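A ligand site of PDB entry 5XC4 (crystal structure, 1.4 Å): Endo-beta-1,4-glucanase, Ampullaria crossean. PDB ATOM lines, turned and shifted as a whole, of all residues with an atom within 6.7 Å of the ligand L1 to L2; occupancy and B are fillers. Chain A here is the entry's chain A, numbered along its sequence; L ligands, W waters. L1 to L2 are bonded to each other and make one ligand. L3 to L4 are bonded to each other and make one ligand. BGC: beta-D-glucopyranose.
The backbone carbonyl oxygen (O) of Ala 111 lies close to an oxygen (O5) of BGC L1 (3.5 Å).
CB of His 34 touches O3 of BGC L1, at 3.4 Å.
CB of Ala 37 touches O4 of BGC L1, at 3.6 Å.
CE3 of Trp 73 touches O3 of BGC L2 (3.5 Å).
CD of Pro 113 touches O5 of BGC L1, 3.7 Å away.
Hydrophobic or aromatic side chains within 4 Å of the ligand L1 to L2: His 34, Ala 37, Leu 72, Trp 73 and Pro 113.
Within 4 Å of the ligand L1 to L2: Asp 32, His 34, Lys 35, Gly 36, Ala 37, Asp 46, Leu 72, Trp 73, Asn 110, Ala 111 and Pro 113.
The nearest printed residue that does not touch the ligand L1 to L2 is Tyr 30 (4.5 Å).
The side-chain carboxylate of Asp 32 is in hydrogen-bond range of an oxygen (O2) of BGC L1 (2.6 Å).
The side-chain carboxylate (OD1) of Asp 46 is in hydrogen-bond range of an oxygen (O6) of BGC L2 (2.7 Å).
O of Leu 72 lies within hydrogen-bond range of O2 of BGC L2.
An oxygen (O2) of BGC L1 is in hydrogen-bond range of the side-chain amide nitrogen (ND2) of Asn 110 (2.8 Å).
The backbone NH (N) of Gly 36 sits at hydrogen-bond distance from an oxygen (O6) of BGC L2 (2.9 Å).
N of Lys 35 sits at hydrogen-bond distance from O6 of BGC L2 (3.5 Å).
OD1 of Asn 117 lies within hydrogen-bond range of O6 of BGC L4, 2.8 Å away.
The side-chain carboxylate (OD2) of Asp 142 is in hydrogen-bond range of an oxygen (O4) of BGC L4, at 2.6 Å.
The backbone NH (N) of His 34 lies within hydrogen-bond range of the side-chain carboxylate (OD1) of Asp 32.
OD2 of Asp 46 sits at hydrogen-bond distance from ND1 of His 34 (2.6 Å).
OD1 of Asp 46 lies within hydrogen-bond range of N of Lys 35, at 3.0 Å.
N of Ala 37 sits at hydrogen-bond distance from OD1 of Asn 110, 2.9 Å away.
O of Ser 45 is in hydrogen-bond range of NZ of Lys 35 (2.7 Å).
NE1 of Trp 73 lies within hydrogen-bond range of SG of Cys 74, at 3.6 Å.
N of Cys 74 lies within hydrogen-bond range of O of Ala 37, at 2.9 Å.
O of Pro 113 sits at hydrogen-bond distance from ND2 of Asn 117 (3.1 Å).
Water W3 bridges O1 of BGC L1 and O of Ala 111.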
ATOM      1  N   TYR A  30      20.638  -2.780  18.164  1.00  0.00           N
ATOM      2  CA  TYR A  30      21.456  -3.001  16.990  1.00  0.00           C
ATOM      3  C   TYR A  30      20.864  -4.139  16.174  1.00  0.00           C
ATOM      4  O   TYR A  30      20.135  -4.989  16.682  1.00  0.00           O
ATOM      5  CB  TYR A  30      22.912  -3.375  17.332  1.00  0.00           C
ATOM      6  CG  TYR A  30      23.193  -4.778  17.833  1.00  0.00           C
ATOM      7  CD1 TYR A  30      22.878  -5.203  19.115  1.00  0.00           C
ATOM      8  CD2 TYR A  30      23.828  -5.692  17.007  1.00  0.00           C
ATOM      9  CE1 TYR A  30      23.208  -6.476  19.581  1.00  0.00           C
ATOM     10  CE2 TYR A  30      24.148  -6.990  17.439  1.00  0.00           C
ATOM     11  CZ  TYR A  30      23.861  -7.363  18.730  1.00  0.00           C
ATOM     12  OH  TYR A  30      24.204  -8.641  19.148  1.00  0.00           O
ATOM     13  N   ASP A  32      22.629  -6.666  13.024  1.00  0.00           N
ATOM     14  CA  ASP A  32      23.725  -6.911  12.068  1.00  0.00           C
ATOM     15  C   ASP A  32      23.746  -8.295  11.453  1.00  0.00           C
ATOM     16  O   ASP A  32      24.497  -8.498  10.474  1.00  0.00           O
ATOM     17  CB  ASP A  32      25.121  -6.511  12.605  1.00  0.00           C
ATOM     18  CG  ASP A  32      25.588  -7.375  13.785  1.00  0.00           C
ATOM     19  OD1 ASP A  32      25.095  -8.517  13.978  1.00  0.00           O
ATOM     20  OD2 ASP A  32      26.506  -6.887  14.490  1.00  0.00           O
ATOM     21  N   GLY A  33      22.980  -9.261  12.010  1.00  0.00           N
ATOM     22  CA  GLY A  33      22.879 -10.614  11.464  1.00  0.00           C
ATOM     23  C   GLY A  33      24.058 -11.543  11.705  1.00  0.00           C
ATOM     24  O   GLY A  33      24.018 -12.693  11.244  1.00  0.00           O
ATOM     25  N   HIS A  34      25.110 -11.100  12.391  1.00  0.00           N
ATOM     26  CA  HIS A  34      26.276 -11.956  12.620  1.00  0.00           C
ATOM     27  C   HIS A  34      25.988 -12.997  13.685  1.00  0.00           C
ATOM     28  O   HIS A  34      25.125 -12.832  14.550  1.00  0.00           O
ATOM     29  CB  HIS A  34      27.442 -11.099  13.121  1.00  0.00           C
ATOM     30  CG  HIS A  34      27.987 -10.187  12.079  1.00  0.00           C
ATOM     31  ND1 HIS A  34      28.508 -10.649  10.887  1.00  0.00           N
ATOM     32  CD2 HIS A  34      28.124  -8.839  12.053  1.00  0.00           C
ATOM     33  CE1 HIS A  34      28.936  -9.626  10.164  1.00  0.00           C
ATOM     34  NE2 HIS A  34      28.709  -8.515  10.857  1.00  0.00           N
ATOM     35  N   LYS A  35      26.767 -14.087  13.628  1.00  0.00           N
ATOM     36  CA  LYS A  35      26.713 -15.092  14.664  1.00  0.00           C
ATOM     37  C   LYS A  35      27.053 -14.482  16.025  1.00  0.00           C
ATOM     38  O   LYS A  35      26.351 -14.730  17.020  1.00  0.00           O
ATOM     39  CB  LYS A  35      27.711 -16.190  14.331  1.00  0.00           C
ATOM     40  CG  LYS A  35      27.817 -17.239  15.481  1.00  0.00           C
ATOM     41  CD  LYS A  35      28.530 -18.518  14.992  1.00  0.00           C
ATOM     42  CE  LYS A  35      30.010 -18.250  14.693  1.00  0.00           C
ATOM     43  NZ  LYS A  35      30.601 -19.524  14.205  1.00  0.00           N
ATOM     44  N   GLY A  36      28.113 -13.699  16.079  1.00  0.00           N
ATOM     45  CA  GLY A  36      28.450 -12.963  17.284  1.00  0.00           C
ATOM     46  C   GLY A  36      29.568 -13.639  18.084  1.00  0.00           C
ATOM     47  O   GLY A  36      29.996 -14.773  17.815  1.00  0.00           O
ATOM     48  N   ALA A  37      30.039 -12.873  19.080  1.00  0.00           N
ATOM     49  CA  ALA A  37      31.307 -13.143  19.750  1.00  0.00           C
ATOM     50  C   ALA A  37      31.255 -14.275  20.772  1.00  0.00           C
ATOM     51  O   ALA A  37      32.318 -14.641  21.306  1.00  0.00           O
ATOM     52  CB  ALA A  37      31.774 -11.843  20.415  1.00  0.00           C
ATOM     53  N   CYS A  38      30.084 -14.862  21.054  1.00  0.00           N
ATOM     54  CA  CYS A  38      30.005 -16.011  21.932  1.00  0.00           C
ATOM     55  C   CYS A  38      29.753 -17.297  21.134  1.00  0.00           C
ATOM     56  O   CYS A  38      29.551 -18.388  21.732  1.00  0.00           O
ATOM     57  CB  CYS A  38      28.940 -15.805  23.024  1.00  0.00           C
ATOM     58  SG  CYS A  38      29.269 -14.411  24.090  1.00  0.00           S
ATOM     59  N   GLY A  39      29.822 -17.217  19.797  1.00  0.00           N
ATOM     60  CA  GLY A  39      29.724 -18.445  19.005  1.00  0.00           C
ATOM     61  C   GLY A  39      28.357 -19.097  19.057  1.00  0.00           C
ATOM     62  O   GLY A  39      28.260 -20.319  18.898  1.00  0.00           O
ATOM     63  N   SER A  45      30.866 -21.011  10.585  1.00  0.00           N
ATOM     64  CA  SER A  45      30.027 -20.136   9.779  1.00  0.00           C
ATOM     65  C   SER A  45      29.834 -18.819  10.504  1.00  0.00           C
ATOM     66  O   SER A  45      30.137 -18.681  11.703  1.00  0.00           O
ATOM     67  CB  SER A  45      28.644 -20.772   9.585  1.00  0.00           C
ATOM     68  OG  SER A  45      27.835 -20.466  10.726  1.00  0.00           O
ATOM     69  N   ASP A  46      29.319 -17.828   9.796  1.00  0.00           N
ATOM     70  CA  ASP A  46      28.845 -16.603  10.450  1.00  0.00           C
ATOM     71  C   ASP A  46      27.334 -16.569  10.542  1.00  0.00           C
ATOM     72  O   ASP A  46      26.711 -15.506  10.395  1.00  0.00           O
ATOM     73  CB  ASP A  46      29.395 -15.356   9.753  1.00  0.00           C
ATOM     74  CG  ASP A  46      29.161 -14.071  10.566  1.00  0.00           C
ATOM     75  OD1 ASP A  46      29.079 -14.139  11.786  1.00  0.00           O
ATOM     76  OD2 ASP A  46      29.004 -12.992   9.957  1.00  0.00           O
ATOM     77  N   THR A  47      26.717 -17.710  10.810  1.00  0.00           N
ATOM     78  CA  THR A  47      25.253 -17.824  10.822  1.00  0.00           C
ATOM     79  C   THR A  47      24.783 -18.040  12.241  1.00  0.00           C
ATOM     80  O   THR A  47      25.154 -19.065  12.835  1.00  0.00           O
ATOM     81  CB  THR A  47      24.829 -19.036   9.988  1.00  0.00           C
ATOM     82  OG1 THR A  47      25.335 -18.853   8.659  1.00  0.00           O
ATOM     83  CG2 THR A  47      23.295 -19.134   9.958  1.00  0.00           C
ATOM     84  N   ALA A  59      24.692  -7.425  23.475  1.00  0.00           N
ATOM     85  CA  ALA A  59      26.137  -7.244  23.286  1.00  0.00           C
ATOM     86  C   ALA A  59      26.584  -6.155  24.252  1.00  0.00           C
ATOM     87  O   ALA A  59      26.400  -4.974  23.954  1.00  0.00           O
ATOM     88  CB  ALA A  59      26.408  -6.808  21.842  1.00  0.00           C
ATOM     89  N   ASN A  71      39.518  -9.710  24.802  1.00  0.00           N
ATOM     90  CA  ASN A  71      39.153 -10.781  23.881  1.00  0.00           C
ATOM     91  C   ASN A  71      37.747 -10.579  23.353  1.00  0.00           C
ATOM     92  O   ASN A  71      36.808 -10.372  24.123  1.00  0.00           O
ATOM     93  CB  ASN A  71      39.189 -12.137  24.575  1.00  0.00           C
ATOM     94  CG  ASN A  71      40.560 -12.566  24.874  1.00  0.00           C
ATOM     95  OD1 ASN A  71      41.396 -12.605  23.995  1.00  0.00           O
ATOM     96  ND2 ASN A  71      40.826 -12.821  26.145  1.00  0.00           N
ATOM     97  N   LEU A  72      37.607 -10.626  22.028  1.00  0.00           N
ATOM     98  CA  LEU A  72      36.317 -10.469  21.365  1.00  0.00           C
ATOM     99  C   LEU A  72      35.812 -11.786  20.800  1.00  0.00           C
ATOM    100  O   LEU A  72      34.977 -11.802  19.904  1.00  0.00           O
ATOM    101  CB  LEU A  72      36.411  -9.404  20.272  1.00  0.00           C
ATOM    102  CG  LEU A  72      36.667  -7.984  20.830  1.00  0.00           C
ATOM    103  CD1 LEU A  72      36.945  -7.021  19.670  1.00  0.00           C
ATOM    104  CD2 LEU A  72      35.461  -7.519  21.693  1.00  0.00           C
ATOM    105  N   TRP A  73      36.265 -12.901  21.382  1.00  0.00           N
ATOM    106  CA  TRP A  73      35.769 -14.234  21.046  1.00  0.00           C
ATOM    107  C   TRP A  73      35.779 -15.027  22.343  1.00  0.00           C
ATOM    108  O   TRP A  73      36.818 -15.117  22.998  1.00  0.00           O
ATOM    109  CB  TRP A  73      36.680 -14.904  19.993  1.00  0.00           C
ATOM    110  CG  TRP A  73      36.315 -16.353  19.671  1.00  0.00           C
ATOM    111  CD1 TRP A  73      37.023 -17.462  20.019  1.00  0.00           C
ATOM    112  CD2 TRP A  73      35.106 -16.825  19.023  1.00  0.00           C
ATOM    113  NE1 TRP A  73      36.366 -18.594  19.590  1.00  0.00           N
ATOM    114  CE2 TRP A  73      35.188 -18.236  18.987  1.00  0.00           C
ATOM    115  CE3 TRP A  73      33.998 -16.199  18.446  1.00  0.00           C
ATOM    116  CZ2 TRP A  73      34.209 -19.021  18.401  1.00  0.00           C
ATOM    117  CZ3 TRP A  73      32.993 -17.009  17.881  1.00  0.00           C
ATOM    118  CH2 TRP A  73      33.147 -18.391  17.826  1.00  0.00           C
ATOM    119  N   CYS A  74      34.619 -15.548  22.739  1.00  0.00           N
ATOM    120  CA  CYS A  74      34.465 -16.269  24.003  1.00  0.00           C
ATOM    121  C   CYS A  74      34.962 -15.421  25.157  1.00  0.00           C
ATOM    122  O   CYS A  74      35.797 -15.829  25.969  1.00  0.00           O
ATOM    123  CB  CYS A  74      35.163 -17.646  23.967  1.00  0.00           C
ATOM    124  SG  CYS A  74      34.573 -18.767  22.679  1.00  0.00           S
ATOM    125  N   ASN A 110      27.066 -11.560  22.620  1.00  0.00           N
ATOM    126  CA  ASN A 110      27.892 -10.850  21.646  1.00  0.00           C
ATOM    127  C   ASN A 110      28.611  -9.751  22.403  1.00  0.00           C
ATOM    128  O   ASN A 110      28.396  -9.564  23.606  1.00  0.00           O
ATOM    129  CB  ASN A 110      26.979 -10.355  20.519  1.00  0.00           C
ATOM    130  CG  ASN A 110      27.733  -9.947  19.275  1.00  0.00           C
ATOM    131  OD1 ASN A 110      28.936 -10.187  19.102  1.00  0.00           O
ATOM    132  ND2 ASN A 110      27.014  -9.287  18.361  1.00  0.00           N
ATOM    133  N   ALA A 111      29.428  -8.983  21.697  1.00  0.00           N
ATOM    134  CA  ALA A 111      30.217  -7.900  22.287  1.00  0.00           C
ATOM    135  C   ALA A 111      30.017  -6.621  21.493  1.00  0.00           C
ATOM    136  O   ALA A 111      29.878  -6.647  20.260  1.00  0.00           O
ATOM    137  CB  ALA A 111      31.728  -8.224  22.273  1.00  0.00           C
ATOM    138  N   CYS A 112      30.057  -5.498  22.200  1.00  0.00           N
ATOM    139  CA  CYS A 112      30.095  -4.167  21.596  1.00  0.00           C
ATOM    140  C   CYS A 112      31.518  -3.641  21.744  1.00  0.00           C
ATOM    141  O   CYS A 112      31.901  -3.204  22.837  1.00  0.00           O
ATOM    142  CB  CYS A 112      29.113  -3.273  22.332  1.00  0.00           C
ATOM    143  SG  CYS A 112      29.025  -1.579  21.575  1.00  0.00           S
ATOM    144  N   PRO A 113      32.326  -3.671  20.685  1.00  0.00           N
ATOM    145  CA  PRO A 113      33.748  -3.309  20.819  1.00  0.00           C
ATOM    146  C   PRO A 113      33.922  -1.805  20.966  1.00  0.00           C
ATOM    147  O   PRO A 113      33.115  -1.023  20.472  1.00  0.00           O
ATOM    148  CB  PRO A 113      34.373  -3.802  19.509  1.00  0.00           C
ATOM    149  CG  PRO A 113      33.206  -3.842  18.543  1.00  0.00           C
ATOM    150  CD  PRO A 113      31.982  -4.192  19.338  1.00  0.00           C
ATOM    151  N   ASN A 117      32.554   2.150  18.265  1.00  0.00           N
ATOM    152  CA  ASN A 117      31.421   2.408  19.142  1.00  0.00           C
ATOM    153  C   ASN A 117      31.882   3.243  20.321  1.00  0.00           C
ATOM    154  O   ASN A 117      31.602   2.946  21.469  1.00  0.00           O
ATOM    155  CB  ASN A 117      30.824   1.107  19.647  1.00  0.00           C
ATOM    156  CG  ASN A 117      30.291   0.258  18.537  1.00  0.00           C
ATOM    157  OD1 ASN A 117      29.222   0.517  17.998  1.00  0.00           O
ATOM    158  ND2 ASN A 117      31.022  -0.791  18.191  1.00  0.00           N
ATOM    159  N   ASP A 142      24.071  -3.125  24.344  1.00  0.00           N
ATOM    160  CA  ASP A 142      23.472  -3.010  23.008  1.00  0.00           C
ATOM    161  C   ASP A 142      22.489  -4.172  22.862  1.00  0.00           C
ATOM    162  O   ASP A 142      22.876  -5.333  23.037  1.00  0.00           O
ATOM    163  CB  ASP A 142      24.589  -3.090  21.972  1.00  0.00           C
ATOM    164  CG  ASP A 142      24.322  -2.371  20.693  1.00  0.00           C
ATOM    165  OD1 ASP A 142      23.263  -1.732  20.571  1.00  0.00           O
ATOM    166  OD2 ASP A 142      25.205  -2.480  19.797  1.00  0.00           O
HETATM  167  C2  BGC L   1      29.479  -8.201  15.885  1.00  0.00           C
HETATM  168  C3  BGC L   1      30.243  -9.483  16.169  1.00  0.00           C
HETATM  169  C4  BGC L   1      31.715  -9.220  16.518  1.00  0.00           C
HETATM  170  C5  BGC L   1      31.832  -8.159  17.608  1.00  0.00           C
HETATM  171  C6  BGC L   1      33.301  -7.845  17.922  1.00  0.00           C
HETATM  172  C1  BGC L   1      29.787  -7.202  17.004  1.00  0.00           C
HETATM  173  O1  BGC L   1      29.118  -5.954  16.765  1.00  0.00           O
HETATM  174  O2  BGC L   1      28.077  -8.529  15.836  1.00  0.00           O
HETATM  175  O3  BGC L   1      30.118 -10.357  15.010  1.00  0.00           O
HETATM  176  O4  BGC L   1      32.299 -10.388  17.113  1.00  0.00           O
HETATM  177  O5  BGC L   1      31.209  -6.993  17.094  1.00  0.00           O
HETATM  178  O6  BGC L   1      33.955  -7.315  16.751  1.00  0.00           O
HETATM  179  C2  BGC L   2      34.043 -12.028  16.882  1.00  0.00           C
HETATM  180  C3  BGC L   2      34.677 -12.989  15.895  1.00  0.00           C
HETATM  181  C4  BGC L   2      33.614 -13.937  15.381  1.00  0.00           C
HETATM  182  C5  BGC L   2      32.421 -13.172  14.818  1.00  0.00           C
HETATM  183  C6  BGC L   2      31.292 -14.108  14.419  1.00  0.00           C
HETATM  184  C1  BGC L   2      32.889 -11.320  16.199  1.00  0.00           C
HETATM  185  O2  BGC L   2      35.016 -11.079  17.293  1.00  0.00           O
HETATM  186  O3  BGC L   2      35.711 -13.752  16.541  1.00  0.00           O
HETATM  187  O4  BGC L   2      34.180 -14.733  14.317  1.00  0.00           O
HETATM  188  O5  BGC L   2      31.912 -12.312  15.850  1.00  0.00           O
HETATM  189  O6  BGC L   2      30.136 -13.308  14.094  1.00  0.00           O
HETATM  190  C2  BGC L   3      21.998   6.652  18.963  1.00  0.00           C
HETATM  191  C3  BGC L   3      22.811   5.629  18.182  1.00  0.00           C
HETATM  192  C4  BGC L   3      22.195   4.213  18.264  1.00  0.00           C
HETATM  193  C5  BGC L   3      20.710   4.305  17.923  1.00  0.00           C
HETATM  194  C6  BGC L   3      19.915   3.037  18.181  1.00  0.00           C
HETATM  195  C1  BGC L   3      20.570   6.599  18.484  1.00  0.00           C
HETATM  196  O1  BGC L   3      19.727   7.434  19.274  1.00  0.00           O
HETATM  197  O2  BGC L   3      22.410   8.020  18.698  1.00  0.00           O
HETATM  198  O3  BGC L   3      24.169   5.677  18.632  1.00  0.00           O
HETATM  199  O4  BGC L   3      22.856   3.403  17.270  1.00  0.00           O
HETATM  200  O5  BGC L   3      20.119   5.289  18.764  1.00  0.00           O
HETATM  201  O6  BGC L   3      20.143   2.510  19.493  1.00  0.00           O
HETATM  202  C2  BGC L   4      23.511   1.285  16.493  1.00  0.00           C
HETATM  203  C3  BGC L   4      24.249   0.007  16.830  1.00  0.00           C
HETATM  204  C4  BGC L   4      25.520   0.327  17.626  1.00  0.00           C
HETATM  205  C5  BGC L   4      25.113   1.092  18.890  1.00  0.00           C
HETATM  206  C6  BGC L   4      26.238   1.469  19.863  1.00  0.00           C
HETATM  207  C1  BGC L   4      23.307   2.124  17.734  1.00  0.00           C
HETATM  208  O2  BGC L   4      22.228   0.958  15.935  1.00  0.00           O
HETATM  209  O3  BGC L   4      24.579  -0.623  15.582  1.00  0.00           O
HETATM  210  O4  BGC L   4      26.150  -0.898  18.014  1.00  0.00           O
HETATM  211  O5  BGC L   4      24.526   2.332  18.456  1.00  0.00           O
HETATM  212  O6  BGC L   4      27.266   2.152  19.129  1.00  0.00           O
HETATM  213  O   HOH W   1      38.098 -12.498  17.151  1.00  0.00           O
HETATM  214  O   HOH W   2      37.361 -15.164  14.712  1.00  0.00           O
HETATM  215  O   HOH W   3      28.487  -3.959  18.538  1.00  0.00           O
HETATM  216  O   HOH W   4      31.720  -9.821  12.632  1.00  0.00           O
